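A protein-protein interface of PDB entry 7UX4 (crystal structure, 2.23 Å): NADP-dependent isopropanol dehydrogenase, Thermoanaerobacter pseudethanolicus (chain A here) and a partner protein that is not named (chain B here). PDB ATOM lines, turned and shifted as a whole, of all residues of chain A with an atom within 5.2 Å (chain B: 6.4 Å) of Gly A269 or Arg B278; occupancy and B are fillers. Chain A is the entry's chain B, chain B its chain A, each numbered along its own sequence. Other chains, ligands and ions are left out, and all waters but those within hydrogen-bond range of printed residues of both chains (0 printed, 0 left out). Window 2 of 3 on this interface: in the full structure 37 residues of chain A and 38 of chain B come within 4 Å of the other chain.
The backbone carbonyl oxygen of Gly A271 sits at hydrogen-bond distance from the guanidinium group of Arg B278, at 2.6 Å.
O of Phe A268 lies within hydrogen-bond range of NH1 of Arg B278.
NH1 of Arg B278 lies close to O of Gly A269.
O of Val B276 sits at hydrogen-bond distance from N of Leu A274, 2.8 Å away.
The backbone carbonyl oxygen (O) of Glu A272 sits at hydrogen-bond distance from the backbone NH (N) of Arg B278, at 3.3 Å.
The backbone NH (N) of Phe A268 is in hydrogen-bond range of the backbone carbonyl oxygen (O) of Cys B283 (3.1 Å).
N of Cys B283 lies within hydrogen-bond range of O of Arg B278 (2.8 Å).
Among the printed residues, merely in contact across the chains: Tyr A267 with Cys B283, Glu A270 with Arg B278, Glu A272 with Pro B277, Val A273 with Val B276 and Leu A274 with Trp B281.
Printed residues of chain B within 4 Å of Phe A268: Arg B278 and Cys B283.
Of chain B, only Arg B278 comes within 4 Å of Gly A269.
Of the printed residues of chain B, Gly A271 touches Arg B278 (2.6 Å).
Of the printed residues of chain B, Leu A274 touches Val B276 and Trp B281.
Arg B278 touches just these residues of chain A: Phe A268 (2.9 Å), Gly A269 (3.2 Å), Glu A270 (3.5 Å), Gly A271 (2.6 Å) and Glu A272 (3.3 Å).
Leu B279 touches none of the printed residues of chain A.
Printed residues of chain A within 4 Å of Trp B281: Leu A274 (3.6 Å).
Of the printed residues of chain A, Cys B283 touches Tyr A267 (3.4 Å) and Phe A268 (3.1 Å).
The nearest printed residue of chain A that does not touch Arg B278 is Leu A274 (4.2 Å).
Of the 8 printed residues of chain A, 8 touch a printed residue of chain B.
Hydrophobic or aromatic side chains of chain A within 4 Å of the printed part of chain B: Tyr A267, Phe A268, Val A273 and Leu A274.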
ATOM      1  N   TYR A 267     -27.124   1.780   4.000  1.00  0.00           N
ATOM      2  CA  TYR A 267     -26.380   0.678   4.599  1.00  0.00           C
ATOM      3  C   TYR A 267     -24.936   0.750   4.115  1.00  0.00           C
ATOM      4  O   TYR A 267     -24.654   0.481   2.943  1.00  0.00           O
ATOM      5  CB  TYR A 267     -26.982  -0.674   4.228  1.00  0.00           C
ATOM      6  CG  TYR A 267     -26.055  -1.826   4.568  1.00  0.00           C
ATOM      7  CD1 TYR A 267     -25.380  -1.867   5.782  1.00  0.00           C
ATOM      8  CD2 TYR A 267     -25.784  -2.824   3.639  1.00  0.00           C
ATOM      9  CE1 TYR A 267     -24.513  -2.898   6.084  1.00  0.00           C
ATOM     10  CE2 TYR A 267     -24.910  -3.859   3.936  1.00  0.00           C
ATOM     11  CZ  TYR A 267     -24.278  -3.888   5.162  1.00  0.00           C
ATOM     12  OH  TYR A 267     -23.402  -4.902   5.479  1.00  0.00           O
ATOM     13  N   PHE A 268     -24.026   1.106   5.017  1.00  0.00           N
ATOM     14  CA  PHE A 268     -22.599   1.113   4.718  1.00  0.00           C
ATOM     15  C   PHE A 268     -22.073  -0.286   4.999  1.00  0.00           C
ATOM     16  O   PHE A 268     -21.968  -0.694   6.161  1.00  0.00           O
ATOM     17  CB  PHE A 268     -21.872   2.160   5.556  1.00  0.00           C
ATOM     18  CG  PHE A 268     -22.411   3.548   5.385  1.00  0.00           C
ATOM     19  CD1 PHE A 268     -21.972   4.353   4.347  1.00  0.00           C
ATOM     20  CD2 PHE A 268     -23.364   4.049   6.256  1.00  0.00           C
ATOM     21  CE1 PHE A 268     -22.469   5.633   4.182  1.00  0.00           C
ATOM     22  CE2 PHE A 268     -23.862   5.329   6.099  1.00  0.00           C
ATOM     23  CZ  PHE A 268     -23.413   6.123   5.058  1.00  0.00           C
ATOM     24  N   GLY A 269     -21.755  -1.026   3.939  1.00  0.00           N
ATOM     25  CA  GLY A 269     -21.351  -2.408   4.056  1.00  0.00           C
ATOM     26  C   GLY A 269     -19.876  -2.699   3.943  1.00  0.00           C
ATOM     27  O   GLY A 269     -19.493  -3.872   3.966  1.00  0.00           O
ATOM     28  N   GLU A 270     -19.029  -1.680   3.817  1.00  0.00           N
ATOM     29  CA  GLU A 270     -17.603  -1.932   3.678  1.00  0.00           C
ATOM     30  C   GLU A 270     -16.841  -0.773   4.303  1.00  0.00           C
ATOM     31  O   GLU A 270     -17.308   0.368   4.306  1.00  0.00           O
ATOM     32  CB  GLU A 270     -17.201  -2.142   2.209  1.00  0.00           C
ATOM     33  CG  GLU A 270     -15.764  -2.616   2.022  1.00  0.00           C
ATOM     34  CD  GLU A 270     -15.406  -2.867   0.572  1.00  0.00           C
ATOM     35  OE1 GLU A 270     -16.227  -2.545  -0.313  1.00  0.00           O
ATOM     36  OE2 GLU A 270     -14.313  -3.418   0.321  1.00  0.00           O
ATOM     37  N   GLY A 271     -15.674  -1.083   4.837  1.00  0.00           N
ATOM     38  CA  GLY A 271     -14.849  -0.089   5.490  1.00  0.00           C
ATOM     39  C   GLY A 271     -14.919  -0.195   7.001  1.00  0.00           C
ATOM     40  O   GLY A 271     -15.937  -0.581   7.583  1.00  0.00           O
ATOM     41  N   GLU A 272     -13.813   0.159   7.653  1.00  0.00           N
ATOM     42  CA  GLU A 272     -13.759   0.117   9.107  1.00  0.00           C
ATOM     43  C   GLU A 272     -14.346   1.367   9.752  1.00  0.00           C
ATOM     44  O   GLU A 272     -14.814   1.298  10.892  1.00  0.00           O
ATOM     45  CB  GLU A 272     -12.310  -0.086   9.559  1.00  0.00           C
ATOM     46  CG  GLU A 272     -12.126  -0.331  11.050  1.00  0.00           C
ATOM     47  CD  GLU A 272     -10.674  -0.225  11.484  1.00  0.00           C
ATOM     48  OE1 GLU A 272      -9.785  -0.505  10.652  1.00  0.00           O
ATOM     49  OE2 GLU A 272     -10.416   0.135  12.654  1.00  0.00           O
ATOM     50  N   VAL A 273     -14.362   2.492   9.045  1.00  0.00           N
ATOM     51  CA  VAL A 273     -14.723   3.777   9.629  1.00  0.00           C
ATOM     52  C   VAL A 273     -15.564   4.565   8.634  1.00  0.00           C
ATOM     53  O   VAL A 273     -15.298   4.544   7.428  1.00  0.00           O
ATOM     54  CB  VAL A 273     -13.459   4.568  10.036  1.00  0.00           C
ATOM     55  CG1 VAL A 273     -13.720   6.067  10.034  1.00  0.00           C
ATOM     56  CG2 VAL A 273     -12.962   4.109  11.402  1.00  0.00           C
ATOM     57  N   LEU A 274     -16.590   5.250   9.147  1.00  0.00           N
ATOM     58  CA  LEU A 274     -17.311   6.243   8.368  1.00  0.00           C
ATOM     59  C   LEU A 274     -16.715   7.612   8.663  1.00  0.00           C
ATOM     60  O   LEU A 274     -16.659   8.008   9.836  1.00  0.00           O
ATOM     61  CB  LEU A 274     -18.792   6.240   8.709  1.00  0.00           C
ATOM     62  CG  LEU A 274     -19.552   4.915   8.616  1.00  0.00           C
ATOM     63  CD1 LEU A 274     -21.031   5.163   8.824  1.00  0.00           C
ATOM     64  CD2 LEU A 274     -19.306   4.225   7.286  1.00  0.00           C
ATOM     65  N   VAL B 276     -16.085   7.282  12.848  1.00  0.00           N
ATOM     66  CA  VAL B 276     -17.291   6.648  13.368  1.00  0.00           C
ATOM     67  C   VAL B 276     -17.217   5.170  12.992  1.00  0.00           C
ATOM     68  O   VAL B 276     -17.264   4.834  11.798  1.00  0.00           O
ATOM     69  CB  VAL B 276     -18.565   7.301  12.820  1.00  0.00           C
ATOM     70  CG1 VAL B 276     -19.786   6.505  13.252  1.00  0.00           C
ATOM     71  CG2 VAL B 276     -18.662   8.743  13.298  1.00  0.00           C
ATOM     72  N   PRO B 277     -17.092   4.260  13.958  1.00  0.00           N
ATOM     73  CA  PRO B 277     -16.905   2.841  13.620  1.00  0.00           C
ATOM     74  C   PRO B 277     -18.149   2.274  12.952  1.00  0.00           C
ATOM     75  O   PRO B 277     -19.266   2.429  13.451  1.00  0.00           O
ATOM     76  CB  PRO B 277     -16.634   2.187  14.980  1.00  0.00           C
ATOM     77  CG  PRO B 277     -17.309   3.088  15.965  1.00  0.00           C
ATOM     78  CD  PRO B 277     -17.185   4.482  15.411  1.00  0.00           C
ATOM     79  N   ARG B 278     -17.945   1.620  11.806  1.00  0.00           N
ATOM     80  CA  ARG B 278     -19.072   1.182  10.988  1.00  0.00           C
ATOM     81  C   ARG B 278     -19.910   0.126  11.701  1.00  0.00           C
ATOM     82  O   ARG B 278     -21.129   0.283  11.842  1.00  0.00           O
ATOM     83  CB  ARG B 278     -18.567   0.661   9.642  1.00  0.00           C
ATOM     84  CG  ARG B 278     -19.672   0.307   8.660  1.00  0.00           C
ATOM     85  CD  ARG B 278     -19.104  -0.172   7.331  1.00  0.00           C
ATOM     86  NE  ARG B 278     -18.347  -1.412   7.453  1.00  0.00           N
ATOM     87  CZ  ARG B 278     -18.874  -2.625   7.345  1.00  0.00           C
ATOM     88  NH1 ARG B 278     -20.166  -2.800   7.125  1.00  0.00           N
ATOM     89  NH2 ARG B 278     -18.085  -3.687   7.466  1.00  0.00           N
ATOM     90  N   LEU B 279     -19.277  -0.952  12.169  1.00  0.00           N
ATOM     91  CA  LEU B 279     -20.036  -2.056  12.752  1.00  0.00           C
ATOM     92  C   LEU B 279     -20.766  -1.620  14.014  1.00  0.00           C
ATOM     93  O   LEU B 279     -21.969  -1.865  14.165  1.00  0.00           O
ATOM     94  CB  LEU B 279     -19.109  -3.237  13.051  1.00  0.00           C
ATOM     95  CG  LEU B 279     -18.573  -4.003  11.842  1.00  0.00           C
ATOM     96  CD1 LEU B 279     -17.702  -5.169  12.284  1.00  0.00           C
ATOM     97  CD2 LEU B 279     -19.721  -4.491  10.970  1.00  0.00           C
ATOM     98  N   GLU B 280     -20.058  -0.950  14.925  1.00  0.00           N
ATOM     99  CA  GLU B 280     -20.662  -0.532  16.186  1.00  0.00           C
ATOM    100  C   GLU B 280     -21.661   0.601  16.016  1.00  0.00           C
ATOM    101  O   GLU B 280     -22.407   0.890  16.958  1.00  0.00           O
ATOM    102  CB  GLU B 280     -19.571  -0.128  17.180  1.00  0.00           C
ATOM    103  CG  GLU B 280     -18.741  -1.303  17.689  1.00  0.00           C
ATOM    104  CD  GLU B 280     -17.635  -1.716  16.729  1.00  0.00           C
ATOM    105  OE1 GLU B 280     -17.592  -1.191  15.594  1.00  0.00           O
ATOM    106  OE2 GLU B 280     -16.803  -2.569  17.108  1.00  0.00           O
ATOM    107  N   TRP B 281     -21.693   1.249  14.853  1.00  0.00           N
ATOM    108  CA  TRP B 281     -22.734   2.213  14.536  1.00  0.00           C
ATOM    109  C   TRP B 281     -23.877   1.571  13.768  1.00  0.00           C
ATOM    110  O   TRP B 281     -24.618   2.271  13.066  1.00  0.00           O
ATOM    111  CB  TRP B 281     -22.149   3.386  13.745  1.00  0.00           C
ATOM    112  CG  TRP B 281     -22.923   4.661  13.901  1.00  0.00           C
ATOM    113  CD1 TRP B 281     -23.262   5.270  15.073  1.00  0.00           C
ATOM    114  CD2 TRP B 281     -23.433   5.498  12.853  1.00  0.00           C
ATOM    115  NE1 TRP B 281     -23.962   6.425  14.823  1.00  0.00           N
ATOM    116  CE2 TRP B 281     -24.079   6.589  13.468  1.00  0.00           C
ATOM    117  CE3 TRP B 281     -23.408   5.430  11.458  1.00  0.00           C
ATOM    118  CZ2 TRP B 281     -24.698   7.603  12.735  1.00  0.00           C
ATOM    119  CZ3 TRP B 281     -24.026   6.438  10.730  1.00  0.00           C
ATOM    120  CH2 TRP B 281     -24.660   7.509  11.369  1.00  0.00           C
ATOM    121  N   GLY B 282     -24.020   0.250  13.870  1.00  0.00           N
ATOM    122  CA  GLY B 282     -25.081  -0.452  13.178  1.00  0.00           C
ATOM    123  C   GLY B 282     -24.976  -0.385  11.677  1.00  0.00           C
ATOM    124  O   GLY B 282     -25.992  -0.519  10.986  1.00  0.00           O
ATOM    125  N   CYS B 283     -23.768  -0.174  11.150  1.00  0.00           N
ATOM    126  CA  CYS B 283     -23.556   0.039   9.720  1.00  0.00           C
ATOM    127  C   CYS B 283     -24.409   1.199   9.209  1.00  0.00           C
ATOM    128  O   CYS B 283     -24.839   1.221   8.053  1.00  0.00           O
ATOM    129  CB  CYS B 283     -23.826  -1.242   8.930  1.00  0.00           C
ATOM    130  SG  CYS B 283     -22.892  -2.684   9.515  1.00  0.00           S
ATOM    131  N   GLY B 284     -24.665   2.171  10.082  1.00  0.00           N
ATOM    132  CA  GLY B 284     -25.479   3.317   9.750  1.00  0.00           C
ATOM    133  C   GLY B 284     -26.902   3.272  10.260  1.00  0.00           C
ATOM    134  O   GLY B 284     -27.677   4.186   9.951  1.00  0.00           O
